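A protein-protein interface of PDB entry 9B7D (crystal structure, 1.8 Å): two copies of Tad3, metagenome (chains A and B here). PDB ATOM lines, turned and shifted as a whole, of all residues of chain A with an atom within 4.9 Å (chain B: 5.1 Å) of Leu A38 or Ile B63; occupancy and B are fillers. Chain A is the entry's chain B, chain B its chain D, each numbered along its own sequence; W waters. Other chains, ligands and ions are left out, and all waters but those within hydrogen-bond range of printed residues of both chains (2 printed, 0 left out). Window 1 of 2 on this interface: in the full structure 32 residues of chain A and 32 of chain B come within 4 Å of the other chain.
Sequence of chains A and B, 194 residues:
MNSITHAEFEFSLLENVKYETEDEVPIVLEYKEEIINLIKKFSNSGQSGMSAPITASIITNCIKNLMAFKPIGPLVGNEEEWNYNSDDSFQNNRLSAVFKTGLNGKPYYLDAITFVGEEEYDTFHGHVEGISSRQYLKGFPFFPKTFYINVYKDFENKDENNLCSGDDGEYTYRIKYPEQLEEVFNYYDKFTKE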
ATOM      1  N   GLU A  34     -18.295  -2.174  14.194  1.00  0.00           N
ATOM      2  CA  GLU A  34     -19.474  -2.896  14.662  1.00  0.00           C
ATOM      3  C   GLU A  34     -20.077  -3.747  13.551  1.00  0.00           C
ATOM      4  O   GLU A  34     -20.542  -4.865  13.803  1.00  0.00           O
ATOM      5  CB  GLU A  34     -20.502  -1.909  15.220  1.00  0.00           C
ATOM      6  CG  GLU A  34     -20.093  -1.248  16.549  1.00  0.00           C
ATOM      7  CD  GLU A  34     -19.056  -0.144  16.384  1.00  0.00           C
ATOM      8  OE1 GLU A  34     -18.893   0.378  15.259  1.00  0.00           O
ATOM      9  OE2 GLU A  34     -18.387   0.193  17.383  1.00  0.00           O
ATOM     10  N   ILE A  35     -20.075  -3.239  12.316  1.00  0.00           N
ATOM     11  CA  ILE A  35     -20.568  -4.022  11.186  1.00  0.00           C
ATOM     12  C   ILE A  35     -19.671  -5.229  10.939  1.00  0.00           C
ATOM     13  O   ILE A  35     -20.155  -6.350  10.750  1.00  0.00           O
ATOM     14  CB  ILE A  35     -20.695  -3.138   9.931  1.00  0.00           C
ATOM     15  CG1 ILE A  35     -21.788  -2.087  10.131  1.00  0.00           C
ATOM     16  CG2 ILE A  35     -20.956  -3.985   8.682  1.00  0.00           C
ATOM     17  CD1 ILE A  35     -21.747  -0.956   9.117  1.00  0.00           C
ATOM     18  N   ILE A  36     -18.353  -5.020  10.945  1.00  0.00           N
ATOM     19  CA  ILE A  36     -17.427  -6.123  10.686  1.00  0.00           C
ATOM     20  C   ILE A  36     -17.555  -7.192  11.766  1.00  0.00           C
ATOM     21  O   ILE A  36     -17.573  -8.395  11.473  1.00  0.00           O
ATOM     22  CB  ILE A  36     -15.984  -5.596  10.575  1.00  0.00           C
ATOM     23  CG1 ILE A  36     -15.787  -4.827   9.265  1.00  0.00           C
ATOM     24  CG2 ILE A  36     -14.989  -6.746  10.669  1.00  0.00           C
ATOM     25  CD1 ILE A  36     -15.985  -5.670   8.017  1.00  0.00           C
ATOM     26  N   ASN A  37     -17.662  -6.772  13.031  1.00  0.00           N
ATOM     27  CA  ASN A  37     -17.810  -7.739  14.118  1.00  0.00           C
ATOM     28  C   ASN A  37     -19.081  -8.566  13.966  1.00  0.00           C
ATOM     29  O   ASN A  37     -19.096  -9.753  14.315  1.00  0.00           O
ATOM     30  CB  ASN A  37     -17.803  -7.019  15.467  1.00  0.00           C
ATOM     31  CG  ASN A  37     -16.418  -6.541  15.863  1.00  0.00           C
ATOM     32  OD1 ASN A  37     -15.415  -6.977  15.300  1.00  0.00           O
ATOM     33  ND2 ASN A  37     -16.358  -5.629  16.829  1.00  0.00           N
ATOM     34  N   LEU A  38     -20.153  -7.960  13.449  1.00  0.00           N
ATOM     35  CA  LEU A  38     -21.377  -8.712  13.200  1.00  0.00           C
ATOM     36  C   LEU A  38     -21.194  -9.698  12.053  1.00  0.00           C
ATOM     37  O   LEU A  38     -21.622 -10.858  12.150  1.00  0.00           O
ATOM     38  CB  LEU A  38     -22.532  -7.748  12.921  1.00  0.00           C
ATOM     39  CG  LEU A  38     -23.888  -8.394  12.644  1.00  0.00           C
ATOM     40  CD1 LEU A  38     -24.474  -8.979  13.920  1.00  0.00           C
ATOM     41  CD2 LEU A  38     -24.839  -7.368  12.054  1.00  0.00           C
ATOM     42  N   ILE A  39     -20.555  -9.263  10.962  1.00  0.00           N
ATOM     43  CA  ILE A  39     -20.272 -10.170   9.849  1.00  0.00           C
ATOM     44  C   ILE A  39     -19.398 -11.329  10.311  1.00  0.00           C
ATOM     45  O   ILE A  39     -19.622 -12.483   9.923  1.00  0.00           O
ATOM     46  CB  ILE A  39     -19.620  -9.407   8.679  1.00  0.00           C
ATOM     47  CG1 ILE A  39     -20.459  -8.190   8.276  1.00  0.00           C
ATOM     48  CG2 ILE A  39     -19.347 -10.336   7.501  1.00  0.00           C
ATOM     49  CD1 ILE A  39     -21.701  -8.523   7.495  1.00  0.00           C
ATOM     50  N   LYS A  40     -18.387 -11.041  11.136  1.00  0.00           N
ATOM     51  CA  LYS A  40     -17.491 -12.085  11.633  1.00  0.00           C
ATOM     52  C   LYS A  40     -18.257 -13.161  12.393  1.00  0.00           C
ATOM     53  O   LYS A  40     -18.030 -14.361  12.196  1.00  0.00           O
ATOM     54  CB  LYS A  40     -16.419 -11.471  12.537  1.00  0.00           C
ATOM     55  CG  LYS A  40     -15.200 -10.915  11.823  1.00  0.00           C
ATOM     56  CD  LYS A  40     -14.186 -10.416  12.850  1.00  0.00           C
ATOM     57  CE  LYS A  40     -13.075  -9.608  12.205  1.00  0.00           C
ATOM     58  NZ  LYS A  40     -11.909  -9.446  13.119  1.00  0.00           N
ATOM     59  N   LYS A  41     -19.152 -12.748  13.291  1.00  0.00           N
ATOM     60  CA  LYS A  41     -19.938 -13.716  14.050  1.00  0.00           C
ATOM     61  C   LYS A  41     -20.849 -14.515  13.129  1.00  0.00           C
ATOM     62  O   LYS A  41     -20.968 -15.739  13.266  1.00  0.00           O
ATOM     63  CB  LYS A  41     -20.754 -12.990  15.124  1.00  0.00           C
ATOM     64  CG  LYS A  41     -21.575 -13.911  16.014  1.00  0.00           C
ATOM     65  CD  LYS A  41     -20.711 -14.545  17.096  1.00  0.00           C
ATOM     66  CE  LYS A  41     -21.574 -15.239  18.137  1.00  0.00           C
ATOM     67  NZ  LYS A  41     -20.800 -15.553  19.370  1.00  0.00           N
ATOM     68  N   PHE A  42     -21.495 -13.832  12.184  1.00  0.00           N
ATOM     69  CA  PHE A  42     -22.331 -14.494  11.186  1.00  0.00           C
ATOM     70  C   PHE A  42     -21.530 -15.514  10.385  1.00  0.00           C
ATOM     71  O   PHE A  42     -22.009 -16.626  10.119  1.00  0.00           O
ATOM     72  CB  PHE A  42     -22.932 -13.427  10.274  1.00  0.00           C
ATOM     73  CG  PHE A  42     -23.828 -13.957   9.187  1.00  0.00           C
ATOM     74  CD1 PHE A  42     -25.005 -14.627   9.493  1.00  0.00           C
ATOM     75  CD2 PHE A  42     -23.520 -13.728   7.857  1.00  0.00           C
ATOM     76  CE1 PHE A  42     -25.844 -15.080   8.483  1.00  0.00           C
ATOM     77  CE2 PHE A  42     -24.358 -14.171   6.851  1.00  0.00           C
ATOM     78  CZ  PHE A  42     -25.520 -14.849   7.163  1.00  0.00           C
ATOM     79  N   ILE A  59     -31.477 -11.499  11.254  1.00  0.00           N
ATOM     80  CA  ILE A  59     -30.584 -10.563  11.937  1.00  0.00           C
ATOM     81  C   ILE A  59     -30.889  -9.124  11.537  1.00  0.00           C
ATOM     82  O   ILE A  59     -31.058  -8.247  12.395  1.00  0.00           O
ATOM     83  CB  ILE A  59     -29.116 -10.916  11.644  1.00  0.00           C
ATOM     84  CG1 ILE A  59     -28.778 -12.305  12.194  1.00  0.00           C
ATOM     85  CG2 ILE A  59     -28.180  -9.832  12.202  1.00  0.00           C
ATOM     86  CD1 ILE A  59     -27.358 -12.764  11.857  1.00  0.00           C
ATOM     87  N   THR A  60     -30.932  -8.847  10.230  1.00  0.00           N
ATOM     88  CA  THR A  60     -31.061  -7.460   9.795  1.00  0.00           C
ATOM     89  C   THR A  60     -32.448  -6.903  10.095  1.00  0.00           C
ATOM     90  O   THR A  60     -32.583  -5.709  10.395  1.00  0.00           O
ATOM     91  CB  THR A  60     -30.741  -7.327   8.304  1.00  0.00           C
ATOM     92  OG1 THR A  60     -31.648  -8.125   7.542  1.00  0.00           O
ATOM     93  CG2 THR A  60     -29.325  -7.798   8.018  1.00  0.00           C
ATOM     94  N   ILE A  63     -32.320  -5.935  13.715  1.00  0.00           N
ATOM     95  CA  ILE A  63     -31.597  -4.677  13.890  1.00  0.00           C
ATOM     96  C   ILE A  63     -32.455  -3.505  13.439  1.00  0.00           C
ATOM     97  O   ILE A  63     -32.521  -2.475  14.116  1.00  0.00           O
ATOM     98  CB  ILE A  63     -30.248  -4.714  13.145  1.00  0.00           C
ATOM     99  CG1 ILE A  63     -29.326  -5.762  13.766  1.00  0.00           C
ATOM    100  CG2 ILE A  63     -29.566  -3.345  13.190  1.00  0.00           C
ATOM    101  CD1 ILE A  63     -28.095  -6.076  12.914  1.00  0.00           C
ATOM    102  N   TYR B  31     -26.641 -13.502  18.356  1.00  0.00           N
ATOM    103  CA  TYR B  31     -26.038 -12.255  17.904  1.00  0.00           C
ATOM    104  C   TYR B  31     -26.300 -11.091  18.854  1.00  0.00           C
ATOM    105  O   TYR B  31     -26.119  -9.932  18.469  1.00  0.00           O
ATOM    106  CB  TYR B  31     -26.538 -11.924  16.495  1.00  0.00           C
ATOM    107  CG  TYR B  31     -26.199 -13.021  15.509  1.00  0.00           C
ATOM    108  CD1 TYR B  31     -27.073 -14.078  15.276  1.00  0.00           C
ATOM    109  CD2 TYR B  31     -24.980 -13.019  14.842  1.00  0.00           C
ATOM    110  CE1 TYR B  31     -26.745 -15.100  14.387  1.00  0.00           C
ATOM    111  CE2 TYR B  31     -24.648 -14.028  13.947  1.00  0.00           C
ATOM    112  CZ  TYR B  31     -25.533 -15.064  13.725  1.00  0.00           C
ATOM    113  OH  TYR B  31     -25.197 -16.065  12.840  1.00  0.00           O
ATOM    114  N   GLU B  34     -23.275  -8.511  19.488  1.00  0.00           N
ATOM    115  CA  GLU B  34     -22.915  -7.714  18.317  1.00  0.00           C
ATOM    116  C   GLU B  34     -24.025  -6.743  17.934  1.00  0.00           C
ATOM    117  O   GLU B  34     -23.747  -5.627  17.475  1.00  0.00           O
ATOM    118  CB  GLU B  34     -22.579  -8.638  17.144  1.00  0.00           C
ATOM    119  CG  GLU B  34     -21.266  -9.379  17.311  1.00  0.00           C
ATOM    120  CD  GLU B  34     -21.385 -10.606  18.204  1.00  0.00           C
ATOM    121  OE1 GLU B  34     -22.522 -11.057  18.471  1.00  0.00           O
ATOM    122  OE2 GLU B  34     -20.336 -11.109  18.655  1.00  0.00           O
ATOM    123  N   ILE B  35     -25.287  -7.155  18.088  1.00  0.00           N
ATOM    124  CA  ILE B  35     -26.400  -6.259  17.794  1.00  0.00           C
ATOM    125  C   ILE B  35     -26.454  -5.130  18.814  1.00  0.00           C
ATOM    126  O   ILE B  35     -26.640  -3.960  18.458  1.00  0.00           O
ATOM    127  CB  ILE B  35     -27.721  -7.047  17.739  1.00  0.00           C
ATOM    128  CG1 ILE B  35     -27.747  -7.947  16.498  1.00  0.00           C
ATOM    129  CG2 ILE B  35     -28.921  -6.106  17.727  1.00  0.00           C
ATOM    130  CD1 ILE B  35     -28.945  -8.893  16.449  1.00  0.00           C
ATOM    131  N   LEU B  38     -23.811  -2.541  18.199  1.00  0.00           N
ATOM    132  CA  LEU B  38     -24.189  -1.678  17.087  1.00  0.00           C
ATOM    133  C   LEU B  38     -25.217  -0.644  17.528  1.00  0.00           C
ATOM    134  O   LEU B  38     -25.113   0.537  17.173  1.00  0.00           O
ATOM    135  CB  LEU B  38     -24.728  -2.528  15.935  1.00  0.00           C
ATOM    136  CG  LEU B  38     -25.235  -1.770  14.711  1.00  0.00           C
ATOM    137  CD1 LEU B  38     -24.104  -0.983  14.062  1.00  0.00           C
ATOM    138  CD2 LEU B  38     -25.903  -2.720  13.723  1.00  0.00           C
ATOM    139  N   ILE B  59     -27.206   2.086   7.539  1.00  0.00           N
ATOM    140  CA  ILE B  59     -26.486   1.026   8.246  1.00  0.00           C
ATOM    141  C   ILE B  59     -27.075  -0.338   7.919  1.00  0.00           C
ATOM    142  O   ILE B  59     -26.355  -1.270   7.540  1.00  0.00           O
ATOM    143  CB  ILE B  59     -26.502   1.274   9.763  1.00  0.00           C
ATOM    144  CG1 ILE B  59     -25.653   2.486  10.127  1.00  0.00           C
ATOM    145  CG2 ILE B  59     -26.002   0.030  10.517  1.00  0.00           C
ATOM    146  CD1 ILE B  59     -25.983   3.029  11.508  1.00  0.00           C
ATOM    147  N   THR B  60     -28.390  -0.491   8.093  1.00  0.00           N
ATOM    148  CA  THR B  60     -28.979  -1.817   7.928  1.00  0.00           C
ATOM    149  C   THR B  60     -28.934  -2.267   6.473  1.00  0.00           C
ATOM    150  O   THR B  60     -28.795  -3.467   6.202  1.00  0.00           O
ATOM    151  CB  THR B  60     -30.415  -1.846   8.469  1.00  0.00           C
ATOM    152  OG1 THR B  60     -31.231  -0.909   7.759  1.00  0.00           O
ATOM    153  CG2 THR B  60     -30.427  -1.497   9.956  1.00  0.00           C
ATOM    154  N   ASN B  61     -29.014  -1.329   5.524  1.00  0.00           N
ATOM    155  CA  ASN B  61     -28.855  -1.705   4.123  1.00  0.00           C
ATOM    156  C   ASN B  61     -27.434  -2.178   3.842  1.00  0.00           C
ATOM    157  O   ASN B  61     -27.232  -3.137   3.087  1.00  0.00           O
ATOM    158  CB  ASN B  61     -29.231  -0.531   3.216  1.00  0.00           C
ATOM    159  CG  ASN B  61     -29.434  -0.950   1.771  1.00  0.00           C
ATOM    160  OD1 ASN B  61     -30.357  -1.700   1.451  1.00  0.00           O
ATOM    161  ND2 ASN B  61     -28.569  -0.462   0.887  1.00  0.00           N
ATOM    162  N   CYS B  62     -26.440  -1.507   4.431  1.00  0.00           N
ATOM    163  CA  CYS B  62     -25.058  -1.973   4.353  1.00  0.00           C
ATOM    164  C   CYS B  62     -24.913  -3.398   4.864  1.00  0.00           C
ATOM    165  O   CYS B  62     -24.305  -4.249   4.202  1.00  0.00           O
ATOM    166  CB  CYS B  62     -24.144  -1.043   5.149  1.00  0.00           C
ATOM    167  SG  CYS B  62     -22.405  -1.476   5.038  1.00  0.00           S
ATOM    168  N   ILE B  63     -25.440  -3.673   6.059  1.00  0.00           N
ATOM    169  CA  ILE B  63     -25.302  -5.016   6.620  1.00  0.00           C
ATOM    170  C   ILE B  63     -25.956  -6.043   5.709  1.00  0.00           C
ATOM    171  O   ILE B  63     -25.385  -7.105   5.441  1.00  0.00           O
ATOM    172  CB  ILE B  63     -25.885  -5.081   8.044  1.00  0.00           C
ATOM    173  CG1 ILE B  63     -25.075  -4.176   8.976  1.00  0.00           C
ATOM    174  CG2 ILE B  63     -25.852  -6.521   8.551  1.00  0.00           C
ATOM    175  CD1 ILE B  63     -25.771  -3.853  10.285  1.00  0.00           C
ATOM    176  N   LYS B  64     -27.150  -5.741   5.204  1.00  0.00           N
ATOM    177  CA  LYS B  64     -27.839  -6.706   4.353  1.00  0.00           C
ATOM    178  C   LYS B  64     -27.038  -7.004   3.095  1.00  0.00           C
ATOM    179  O   LYS B  64     -26.912  -8.167   2.690  1.00  0.00           O
ATOM    180  CB  LYS B  64     -29.234  -6.200   3.999  1.00  0.00           C
ATOM    181  CG  LYS B  64     -30.118  -7.310   3.493  1.00  0.00           C
ATOM    182  CD  LYS B  64     -31.486  -7.275   4.133  1.00  0.00           C
ATOM    183  CE  LYS B  64     -32.055  -8.682   4.174  1.00  0.00           C
ATOM    184  NZ  LYS B  64     -31.076  -9.622   4.826  1.00  0.00           N
ATOM    185  N   ASN B  65     -26.482  -5.970   2.469  1.00  0.00           N
ATOM    186  CA  ASN B  65     -25.683  -6.178   1.267  1.00  0.00           C
ATOM    187  C   ASN B  65     -24.451  -7.018   1.570  1.00  0.00           C
ATOM    188  O   ASN B  65     -24.172  -8.002   0.878  1.00  0.00           O
ATOM    189  CB  ASN B  65     -25.280  -4.834   0.662  1.00  0.00           C
ATOM    190  CG  ASN B  65     -26.380  -4.223  -0.191  1.00  0.00           C
ATOM    191  OD1 ASN B  65     -27.114  -4.935  -0.879  1.00  0.00           O
ATOM    192  ND2 ASN B  65     -26.486  -2.894  -0.166  1.00  0.00           N
ATOM    193  N   LEU B  66     -23.701  -6.646   2.611  1.00  0.00           N
ATOM    194  CA  LEU B  66     -22.450  -7.345   2.893  1.00  0.00           C
ATOM    195  C   LEU B  66     -22.693  -8.806   3.262  1.00  0.00           C
ATOM    196  O   LEU B  66     -21.908  -9.683   2.884  1.00  0.00           O
ATOM    197  CB  LEU B  66     -21.683  -6.623   3.999  1.00  0.00           C
ATOM    198  CG  LEU B  66     -21.083  -5.279   3.562  1.00  0.00           C
ATOM    199  CD1 LEU B  66     -20.296  -4.635   4.704  1.00  0.00           C
ATOM    200  CD2 LEU B  66     -20.204  -5.443   2.318  1.00  0.00           C
ATOM    201  N   MET B  67     -23.776  -9.089   3.994  1.00  0.00           N
ATOM    202  CA  MET B  67     -24.103 -10.473   4.344  1.00  0.00           C
ATOM    203  C   MET B  67     -24.441 -11.317   3.120  1.00  0.00           C
ATOM    204  O   MET B  67     -24.291 -12.545   3.165  1.00  0.00           O
ATOM    205  CB  MET B  67     -25.273 -10.495   5.335  1.00  0.00           C
ATOM    206  CG  MET B  67     -24.971  -9.843   6.685  1.00  0.00           C
ATOM    207  SD  MET B  67     -26.105 -10.346   8.003  1.00  0.00           S
ATOM    208  CE  MET B  67     -25.042 -10.313   9.444  1.00  0.00           C
ATOM    209  N   ALA B  68     -24.881 -10.690   2.029  1.00  0.00           N
ATOM    210  CA  ALA B  68     -25.176 -11.395   0.785  1.00  0.00           C
ATOM    211  C   ALA B  68     -24.028 -11.332  -0.220  1.00  0.00           C
ATOM    212  O   ALA B  68     -24.218 -11.693  -1.385  1.00  0.00           O
ATOM    213  CB  ALA B  68     -26.451 -10.831   0.154  1.00  0.00           C
HETATM  214  O   HOH W   1     -21.350  -5.308  16.460  1.00  0.00           O
HETATM  215  O   HOH W   2     -19.591 -13.015  20.547  1.00  0.00           O
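The side-chain hydroxyl (OG1) of Thr A60 is in hydrogen-bond range of the side-chain amino group (NZ) of Lys B64 (3.2 Å).
Glu A34 touches Leu B38.
Leu A38 touches Ile B63.
CG of Leu A38 touches CE of Met B67, at 3.9 Å.
CB of Leu B66 touches CD1 of Ile A39, at 3.98 Å.
Met B67 touches Ile A39 (CG to CD1, 3.6 Å).
CG of Lys A41 touches CE2 of Tyr B31, at 3.7 Å.
Tyr B31 touches Phe A42 (CE2 to N, 3.6 Å).
Phe A42 touches Met B67.
CG2 of Ile B63 touches CG2 of Thr A60, at 3.7 Å.
Ile A63 touches Leu B38.
Of the printed residues of chain A, Tyr B31 touches Lys A41 (3.7 Å), Phe A42 (3.6 Å) and Ile A59 (3.5 Å).
Ile B59 touches none of the printed residues of chain A.
Of the printed residues of chain A, Thr B60 touches Ile A63 (3.8 Å).
Ile B63 touches just these residues of chain A: Leu A38 and Thr A60.
The nearest printed residue of chain A that does not touch Glu B34 is Glu A34 (4.9 Å).
Of the 12 printed residues of chain A, 9 touch a printed residue of chain B.
Hydrophobic or aromatic side chains of chain A that line the printed part of chain B: Leu A38, Ile A39, Phe A42, Ile A59 and Ile A63.
Along chain A the printed residues that touch a printed residue of chain B span positions 34 to 63.
Hydrophobic or aromatic side chains of chain B within 4 Å of the printed part of chain A: Tyr B31, Ile B35, Leu B38, Ile B63, Leu B66 and Met B67.
Along chain B the printed residues that touch a printed residue of chain A span positions 31 to 67.
Among the printed residues, no Asp or Glu carboxylate lies within 4 Å of a Lys or Arg side-chain nitrogen of the other chain.
Glu A34 touches Leu B38, and with the chains exchanged Leu A38 touches Glu B34.
Leu A38 touches Ile B63, and with the chains exchanged Ile A63 touches Leu B38.
Thr A60 touches Ile B63, and with the chains exchanged Ile A63 touches Thr B60.
Ile A63 touches Ile B35, but with the chains exchanged Ile A35 does not touch Ile B63 (4.1 Å).
Of the 17 pairs that touch across the chains among the printed residues, 6 have their exchanged pair printed and touching as well.
Water W1 lies within hydrogen-bond range of O of Glu B34 (2.6 Å) and O of Glu A34 (2.8 Å).
Water W2 lies within hydrogen-bond range of the side-chain carboxylate (OE2) of Glu B34 (2.8 Å) and the side-chain amino group (NZ) of Lys A41 (3.0 Å).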
